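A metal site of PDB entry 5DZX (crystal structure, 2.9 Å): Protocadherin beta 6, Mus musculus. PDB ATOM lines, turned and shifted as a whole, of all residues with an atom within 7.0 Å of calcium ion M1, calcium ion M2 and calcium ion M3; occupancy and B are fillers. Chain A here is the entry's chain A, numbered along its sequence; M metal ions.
O of Pro 400 lies within hydrogen-bond range of ND2 of Asn 312. The backbone NH (N) of Ala 282 lies within hydrogen-bond range of the side-chain carboxylate (OD2) of Asp 279. The backbone NH (N) of Leu 402 sits at hydrogen-bond distance from the side-chain carboxylate (OD1) of Asp 396 (2.6 Å). OD1 of Asn 314 sits close to OD1 of Asp 313 (3.0 Å). The side-chain carboxylate of Asp 310 sits close to the backbone NH of Ser 346, 3.4 Å away. ND2 of Asn 349 sits at hydrogen-bond distance from OD2 of Asp 310 (2.6 Å).
The nearest printed residue that does not touch calcium ion M1 is Pro 316 (4.3 Å).
Within 4 Å of calcium ion M2: Glu 225, Glu 281, Asp 310, Val 311, Asp 313 and Asp 345. The nearest printed residue that does not touch calcium ion M2 is Asn 314 (4.3 Å).
Along chain A the residues within 4 Å of calcium ion M3 span positions 225 to 314.
Calcium ion M1 is bound by the side-chain carboxylate (OD2) of Asp 345 (2.3 Å), the side-chain amide oxygen (OD1) of Asn 312 (2.3 Å), the backbone carbonyl oxygen (O) of Asn 349 (2.4 Å), the backbone carbonyl oxygen (O) of Asn 314 (2.5 Å), the side-chain carboxylate (OD2) of Asp 343 (2.6 Å), the side-chain carboxylate (OD1) of Asp 343 (2.7 Å) and the side-chain carboxylate (OD2) of Asp 396 (2.8 Å). Calcium ion M1 has seven donor atoms within binding distance.
Calcium ion M2 is bound by O of Val 311, OE2 of Glu 281, OE1 of Glu 225, OD1 of Asp 313, OD1 of Asp 345 and OD1 of Asp 310.
Calcium ion M3 is bound by OD2 of Asp 313 (2.4 Å), OE1 of Glu 281 (2.5 Å) and OD1 of Asp 279 (2.5 Å). Calcium ion M3 has three donor atoms within binding distance. Slightly farther from calcium ion M3 lies OE1 of Glu 225 (3.0 Å). Slightly farther from calcium ion M3 lies the side-chain carboxylate (OE2) of Glu 225 (3.0 Å).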
ATOM      1  N   GLU A 225     -14.885  12.309  29.392  1.00  0.00           N
ATOM      2  CA  GLU A 225     -15.583  12.078  30.650  1.00  0.00           C
ATOM      3  C   GLU A 225     -14.705  11.361  31.675  1.00  0.00           C
ATOM      4  O   GLU A 225     -15.087  11.189  32.832  1.00  0.00           O
ATOM      5  CB  GLU A 225     -16.861  11.263  30.415  1.00  0.00           C
ATOM      6  CG  GLU A 225     -16.618   9.870  29.855  1.00  0.00           C
ATOM      7  CD  GLU A 225     -17.879   9.027  29.832  1.00  0.00           C
ATOM      8  OE1 GLU A 225     -17.809   7.878  29.355  1.00  0.00           O
ATOM      9  OE2 GLU A 225     -18.935   9.507  30.291  1.00  0.00           O
ATOM     10  N   LEU A 278     -16.383  13.156  35.597  1.00  0.00           N
ATOM     11  CA  LEU A 278     -17.436  13.445  34.626  1.00  0.00           C
ATOM     12  C   LEU A 278     -18.092  12.172  34.097  1.00  0.00           C
ATOM     13  O   LEU A 278     -17.606  11.066  34.348  1.00  0.00           O
ATOM     14  CB  LEU A 278     -16.898  14.251  33.462  1.00  0.00           C
ATOM     15  CG  LEU A 278     -16.537  15.708  33.749  1.00  0.00           C
ATOM     16  CD1 LEU A 278     -15.941  16.356  32.520  1.00  0.00           C
ATOM     17  CD2 LEU A 278     -17.782  16.449  34.199  1.00  0.00           C
ATOM     18  N   ASP A 279     -19.186  12.351  33.375  1.00  0.00           N
ATOM     19  CA  ASP A 279     -19.897  11.246  32.757  1.00  0.00           C
ATOM     20  C   ASP A 279     -20.797  11.746  31.633  1.00  0.00           C
ATOM     21  O   ASP A 279     -21.667  12.590  31.859  1.00  0.00           O
ATOM     22  CB  ASP A 279     -20.718  10.475  33.791  1.00  0.00           C
ATOM     23  CG  ASP A 279     -21.279   9.185  33.237  1.00  0.00           C
ATOM     24  OD1 ASP A 279     -20.611   8.140  33.373  1.00  0.00           O
ATOM     25  OD2 ASP A 279     -22.392   9.207  32.653  1.00  0.00           O
ATOM     26  N   PHE A 280     -20.576  11.226  30.427  1.00  0.00           N
ATOM     27  CA  PHE A 280     -21.323  11.651  29.251  1.00  0.00           C
ATOM     28  C   PHE A 280     -22.775  11.196  29.338  1.00  0.00           C
ATOM     29  O   PHE A 280     -23.676  11.861  28.819  1.00  0.00           O
ATOM     30  CB  PHE A 280     -20.670  11.095  27.985  1.00  0.00           C
ATOM     31  CG  PHE A 280     -21.226  11.673  26.709  1.00  0.00           C
ATOM     32  CD1 PHE A 280     -22.319  11.111  26.084  1.00  0.00           C
ATOM     33  CD2 PHE A 280     -20.627  12.778  26.119  1.00  0.00           C
ATOM     34  CE1 PHE A 280     -22.828  11.645  24.906  1.00  0.00           C
ATOM     35  CE2 PHE A 280     -21.135  13.313  24.942  1.00  0.00           C
ATOM     36  CZ  PHE A 280     -22.232  12.744  24.337  1.00  0.00           C
ATOM     37  N   GLU A 281     -23.006  10.061  29.983  1.00  0.00           N
ATOM     38  CA  GLU A 281     -24.342   9.504  30.099  1.00  0.00           C
ATOM     39  C   GLU A 281     -25.215  10.340  31.027  1.00  0.00           C
ATOM     40  O   GLU A 281     -26.439  10.410  30.866  1.00  0.00           O
ATOM     41  CB  GLU A 281     -24.295   8.045  30.577  1.00  0.00           C
ATOM     42  CG  GLU A 281     -23.739   7.050  29.558  1.00  0.00           C
ATOM     43  CD  GLU A 281     -22.240   7.175  29.357  1.00  0.00           C
ATOM     44  OE1 GLU A 281     -21.552   7.682  30.264  1.00  0.00           O
ATOM     45  OE2 GLU A 281     -21.747   6.758  28.289  1.00  0.00           O
ATOM     46  N   ALA A 282     -24.590  10.983  32.004  1.00  0.00           N
ATOM     47  CA  ALA A 282     -25.318  11.822  32.954  1.00  0.00           C
ATOM     48  C   ALA A 282     -25.554  13.214  32.395  1.00  0.00           C
ATOM     49  O   ALA A 282     -26.691  13.625  32.173  1.00  0.00           O
ATOM     50  CB  ALA A 282     -24.556  11.905  34.281  1.00  0.00           C
ATOM     51  N   LEU A 309     -17.005  14.619  25.758  1.00  0.00           N
ATOM     52  CA  LEU A 309     -16.906  13.649  24.673  1.00  0.00           C
ATOM     53  C   LEU A 309     -17.152  12.245  25.196  1.00  0.00           C
ATOM     54  O   LEU A 309     -16.568  11.837  26.196  1.00  0.00           O
ATOM     55  CB  LEU A 309     -15.536  13.737  24.002  1.00  0.00           C
ATOM     56  CG  LEU A 309     -15.189  15.116  23.435  1.00  0.00           C
ATOM     57  CD1 LEU A 309     -13.800  15.110  22.813  1.00  0.00           C
ATOM     58  CD2 LEU A 309     -16.228  15.553  22.417  1.00  0.00           C
ATOM     59  N   ASP A 310     -18.033  11.514  24.521  1.00  0.00           N
ATOM     60  CA  ASP A 310     -18.397  10.170  24.950  1.00  0.00           C
ATOM     61  C   ASP A 310     -17.286   9.160  24.694  1.00  0.00           C
ATOM     62  O   ASP A 310     -16.868   8.959  23.555  1.00  0.00           O
ATOM     63  CB  ASP A 310     -19.668   9.703  24.257  1.00  0.00           C
ATOM     64  CG  ASP A 310     -19.999   8.254  24.563  1.00  0.00           C
ATOM     65  OD1 ASP A 310     -20.661   7.992  25.589  1.00  0.00           O
ATOM     66  OD2 ASP A 310     -19.612   7.368  23.770  1.00  0.00           O
ATOM     67  N   VAL A 311     -16.801   8.550  25.765  1.00  0.00           N
ATOM     68  CA  VAL A 311     -15.812   7.485  25.639  1.00  0.00           C
ATOM     69  C   VAL A 311     -16.501   6.147  25.846  1.00  0.00           C
ATOM     70  O   VAL A 311     -17.302   5.989  26.770  1.00  0.00           O
ATOM     71  CB  VAL A 311     -14.662   7.661  26.664  1.00  0.00           C
ATOM     72  CG1 VAL A 311     -13.670   6.509  26.555  1.00  0.00           C
ATOM     73  CG2 VAL A 311     -13.967   9.000  26.449  1.00  0.00           C
ATOM     74  N   ASN A 312     -16.214   5.180  24.980  1.00  0.00           N
ATOM     75  CA  ASN A 312     -16.851   3.869  25.057  1.00  0.00           C
ATOM     76  C   ASN A 312     -16.355   3.105  26.284  1.00  0.00           C
ATOM     77  O   ASN A 312     -15.566   2.164  26.163  1.00  0.00           O
ATOM     78  CB  ASN A 312     -16.577   3.069  23.781  1.00  0.00           C
ATOM     79  CG  ASN A 312     -17.410   1.804  23.701  1.00  0.00           C
ATOM     80  OD1 ASN A 312     -18.498   1.725  24.257  1.00  0.00           O
ATOM     81  ND2 ASN A 312     -16.891   0.796  23.003  1.00  0.00           N
ATOM     82  N   ASP A 313     -16.817   3.518  27.454  1.00  0.00           N
ATOM     83  CA  ASP A 313     -16.388   2.937  28.719  1.00  0.00           C
ATOM     84  C   ASP A 313     -17.338   1.865  29.230  1.00  0.00           C
ATOM     85  O   ASP A 313     -17.029   1.161  30.188  1.00  0.00           O
ATOM     86  CB  ASP A 313     -16.260   4.034  29.773  1.00  0.00           C
ATOM     87  CG  ASP A 313     -17.581   4.743  30.050  1.00  0.00           C
ATOM     88  OD1 ASP A 313     -18.451   4.738  29.153  1.00  0.00           O
ATOM     89  OD2 ASP A 313     -17.764   5.282  31.164  1.00  0.00           O
ATOM     90  N   ASN A 314     -18.503   1.755  28.596  1.00  0.00           N
ATOM     91  CA  ASN A 314     -19.500   0.780  29.016  1.00  0.00           C
ATOM     92  C   ASN A 314     -19.736  -0.333  27.999  1.00  0.00           C
ATOM     93  O   ASN A 314     -20.044  -0.077  26.836  1.00  0.00           O
ATOM     94  CB  ASN A 314     -20.824   1.482  29.315  1.00  0.00           C
ATOM     95  CG  ASN A 314     -20.678   2.542  30.388  1.00  0.00           C
ATOM     96  OD1 ASN A 314     -21.089   3.692  30.214  1.00  0.00           O
ATOM     97  ND2 ASN A 314     -20.086   2.162  31.517  1.00  0.00           N
ATOM     98  N   ALA A 315     -19.592  -1.578  28.443  1.00  0.00           N
ATOM     99  CA  ALA A 315     -19.810  -2.731  27.577  1.00  0.00           C
ATOM    100  C   ALA A 315     -21.294  -3.084  27.487  1.00  0.00           C
ATOM    101  O   ALA A 315     -22.048  -2.876  28.447  1.00  0.00           O
ATOM    102  CB  ALA A 315     -19.006  -3.932  28.082  1.00  0.00           C
ATOM    103  N   PRO A 316     -21.732  -3.596  26.323  1.00  0.00           N
ATOM    104  CA  PRO A 316     -23.093  -4.060  26.062  1.00  0.00           C
ATOM    105  C   PRO A 316     -23.643  -4.956  27.173  1.00  0.00           C
ATOM    106  O   PRO A 316     -22.901  -5.747  27.744  1.00  0.00           O
ATOM    107  CB  PRO A 316     -22.944  -4.871  24.765  1.00  0.00           C
ATOM    108  CG  PRO A 316     -21.687  -4.370  24.114  1.00  0.00           C
ATOM    109  CD  PRO A 316     -20.931  -3.503  25.081  1.00  0.00           C
ATOM    110  N   ASP A 343     -27.125  -0.628  25.681  1.00  0.00           N
ATOM    111  CA  ASP A 343     -25.823   0.024  25.745  1.00  0.00           C
ATOM    112  C   ASP A 343     -26.005   1.503  26.067  1.00  0.00           C
ATOM    113  O   ASP A 343     -26.566   2.240  25.261  1.00  0.00           O
ATOM    114  CB  ASP A 343     -25.060  -0.147  24.426  1.00  0.00           C
ATOM    115  CG  ASP A 343     -23.565   0.103  24.570  1.00  0.00           C
ATOM    116  OD1 ASP A 343     -23.136   0.682  25.593  1.00  0.00           O
ATOM    117  OD2 ASP A 343     -22.810  -0.265  23.642  1.00  0.00           O
ATOM    118  N   PRO A 344     -25.545   1.941  27.250  1.00  0.00           N
ATOM    119  CA  PRO A 344     -25.739   3.318  27.708  1.00  0.00           C
ATOM    120  C   PRO A 344     -24.937   4.365  26.932  1.00  0.00           C
ATOM    121  O   PRO A 344     -25.318   5.538  26.911  1.00  0.00           O
ATOM    122  CB  PRO A 344     -25.268   3.264  29.166  1.00  0.00           C
ATOM    123  CG  PRO A 344     -24.298   2.147  29.202  1.00  0.00           C
ATOM    124  CD  PRO A 344     -24.835   1.119  28.250  1.00  0.00           C
ATOM    125  N   ASP A 345     -23.838   3.943  26.303  1.00  0.00           N
ATOM    126  CA  ASP A 345     -22.987   4.851  25.543  1.00  0.00           C
ATOM    127  C   ASP A 345     -23.707   5.484  24.359  1.00  0.00           C
ATOM    128  O   ASP A 345     -24.748   4.991  23.919  1.00  0.00           O
ATOM    129  CB  ASP A 345     -21.740   4.115  25.047  1.00  0.00           C
ATOM    130  CG  ASP A 345     -20.854   3.627  26.186  1.00  0.00           C
ATOM    131  OD1 ASP A 345     -20.698   4.362  27.170  1.00  0.00           O
ATOM    132  OD2 ASP A 345     -20.333   2.493  26.074  1.00  0.00           O
ATOM    133  N   SER A 346     -23.157   6.580  23.844  1.00  0.00           N
ATOM    134  CA  SER A 346     -23.753   7.292  22.713  1.00  0.00           C
ATOM    135  C   SER A 346     -22.965   7.044  21.425  1.00  0.00           C
ATOM    136  O   SER A 346     -21.853   6.528  21.464  1.00  0.00           O
ATOM    137  CB  SER A 346     -23.829   8.795  23.010  1.00  0.00           C
ATOM    138  OG  SER A 346     -24.669   9.050  24.122  1.00  0.00           O
ATOM    139  N   ASP A 348     -21.678   5.443  17.954  1.00  0.00           N
ATOM    140  CA  ASP A 348     -21.444   4.062  17.557  1.00  0.00           C
ATOM    141  C   ASP A 348     -20.921   3.241  18.724  1.00  0.00           C
ATOM    142  O   ASP A 348     -20.717   2.040  18.614  1.00  0.00           O
ATOM    143  CB  ASP A 348     -20.464   3.993  16.376  1.00  0.00           C
ATOM    144  CG  ASP A 348     -21.045   4.532  15.080  1.00  0.00           C
ATOM    145  OD1 ASP A 348     -22.265   4.784  15.038  1.00  0.00           O
ATOM    146  OD2 ASP A 348     -20.279   4.698  14.111  1.00  0.00           O
ATOM    147  N   ASN A 349     -20.695   3.907  19.852  1.00  0.00           N
ATOM    148  CA  ASN A 349     -20.299   3.231  21.073  1.00  0.00           C
ATOM    149  C   ASN A 349     -21.515   2.556  21.719  1.00  0.00           C
ATOM    150  O   ASN A 349     -21.377   1.637  22.519  1.00  0.00           O
ATOM    151  CB  ASN A 349     -19.646   4.201  22.057  1.00  0.00           C
ATOM    152  CG  ASN A 349     -18.458   4.937  21.459  1.00  0.00           C
ATOM    153  OD1 ASN A 349     -17.688   4.365  20.697  1.00  0.00           O
ATOM    154  ND2 ASN A 349     -18.308   6.203  21.816  1.00  0.00           N
ATOM    155  N   GLY A 350     -22.696   3.028  21.344  1.00  0.00           N
ATOM    156  CA  GLY A 350     -23.940   2.507  21.881  1.00  0.00           C
ATOM    157  C   GLY A 350     -24.725   1.673  20.887  1.00  0.00           C
ATOM    158  O   GLY A 350     -25.803   1.154  21.209  1.00  0.00           O
ATOM    159  N   ARG A 351     -24.203   1.535  19.679  1.00  0.00           N
ATOM    160  CA  ARG A 351     -24.807   0.681  18.667  1.00  0.00           C
ATOM    161  C   ARG A 351     -24.231  -0.718  18.812  1.00  0.00           C
ATOM    162  O   ARG A 351     -23.014  -0.892  18.897  1.00  0.00           O
ATOM    163  CB  ARG A 351     -24.561   1.205  17.258  1.00  0.00           C
ATOM    164  CG  ARG A 351     -25.318   2.470  16.898  1.00  0.00           C
ATOM    165  CD  ARG A 351     -24.889   2.995  15.536  1.00  0.00           C
ATOM    166  NE  ARG A 351     -25.129   2.026  14.472  1.00  0.00           N
ATOM    167  CZ  ARG A 351     -24.707   2.172  13.219  1.00  0.00           C
ATOM    168  NH1 ARG A 351     -24.975   1.238  12.308  1.00  0.00           N
ATOM    169  NH2 ARG A 351     -24.029   3.249  12.868  1.00  0.00           N
ATOM    170  N   MET A 352     -25.095  -1.724  18.835  1.00  0.00           N
ATOM    171  CA  MET A 352     -24.659  -3.083  19.085  1.00  0.00           C
ATOM    172  C   MET A 352     -25.026  -4.022  17.955  1.00  0.00           C
ATOM    173  O   MET A 352     -26.053  -3.855  17.287  1.00  0.00           O
ATOM    174  CB  MET A 352     -25.249  -3.602  20.392  1.00  0.00           C
ATOM    175  CG  MET A 352     -24.818  -2.842  21.628  1.00  0.00           C
ATOM    176  SD  MET A 352     -25.880  -3.223  23.040  1.00  0.00           S
ATOM    177  CE  MET A 352     -27.416  -2.459  22.504  1.00  0.00           C
ATOM    178  N   ASP A 396     -20.396  -3.969  20.676  1.00  0.00           N
ATOM    179  CA  ASP A 396     -20.687  -2.649  20.157  1.00  0.00           C
ATOM    180  C   ASP A 396     -19.764  -2.312  18.985  1.00  0.00           C
ATOM    181  O   ASP A 396     -18.816  -3.046  18.715  1.00  0.00           O
ATOM    182  CB  ASP A 396     -20.565  -1.588  21.250  1.00  0.00           C
ATOM    183  CG  ASP A 396     -19.252  -1.688  22.015  1.00  0.00           C
ATOM    184  OD1 ASP A 396     -18.310  -2.333  21.512  1.00  0.00           O
ATOM    185  OD2 ASP A 396     -19.164  -1.090  23.107  1.00  0.00           O
ATOM    186  N   LEU A 397     -20.023  -1.194  18.332  1.00  0.00           N
ATOM    187  CA  LEU A 397     -19.218  -0.764  17.190  1.00  0.00           C
ATOM    188  C   LEU A 397     -18.303   0.388  17.550  1.00  0.00           C
ATOM    189  O   LEU A 397     -17.888   1.168  16.685  1.00  0.00           O
ATOM    190  CB  LEU A 397     -20.135  -0.377  16.020  1.00  0.00           C
ATOM    191  CG  LEU A 397     -21.088  -1.476  15.556  1.00  0.00           C
ATOM    192  CD1 LEU A 397     -22.044  -0.942  14.496  1.00  0.00           C
ATOM    193  CD2 LEU A 397     -20.303  -2.662  15.023  1.00  0.00           C
ATOM    194  N   GLY A 398     -17.974   0.499  18.839  1.00  0.00           N
ATOM    195  CA  GLY A 398     -17.142   1.584  19.318  1.00  0.00           C
ATOM    196  C   GLY A 398     -15.653   1.351  19.141  1.00  0.00           C
ATOM    197  O   GLY A 398     -15.237   0.337  18.569  1.00  0.00           O
ATOM    198  N   PRO A 400     -12.210   1.345  21.544  1.00  0.00           N
ATOM    199  CA  PRO A 400     -12.201  -0.027  21.027  1.00  0.00           C
ATOM    200  C   PRO A 400     -13.562  -0.717  21.159  1.00  0.00           C
ATOM    201  O   PRO A 400     -14.489  -0.115  21.703  1.00  0.00           O
ATOM    202  CB  PRO A 400     -11.163  -0.735  21.917  1.00  0.00           C
ATOM    203  CG  PRO A 400     -10.402   0.374  22.591  1.00  0.00           C
ATOM    204  CD  PRO A 400     -11.394   1.472  22.755  1.00  0.00           C
ATOM    205  N   LEU A 402     -16.162  -3.289  22.709  1.00  0.00           N
ATOM    206  CA  LEU A 402     -16.433  -4.014  23.948  1.00  0.00           C
ATOM    207  C   LEU A 402     -17.411  -5.161  23.703  1.00  0.00           C
ATOM    208  O   LEU A 402     -18.419  -4.982  23.012  1.00  0.00           O
ATOM    209  CB  LEU A 402     -16.974  -3.077  25.018  1.00  0.00           C
ATOM    210  CG  LEU A 402     -16.053  -1.919  25.418  1.00  0.00           C
ATOM    211  CD1 LEU A 402     -16.762  -0.951  26.336  1.00  0.00           C
ATOM    212  CD2 LEU A 402     -14.779  -2.444  26.051  1.00  0.00           C
HETATM  213 CA    CA M   1     -20.595   0.745  24.587  1.00  0.00          CA
HETATM  214 CA    CA M   2     -19.342   6.691  27.719  1.00  0.00          CA
HETATM  215 CA    CA M   3     -19.575   6.855  31.508  1.00  0.00          CA
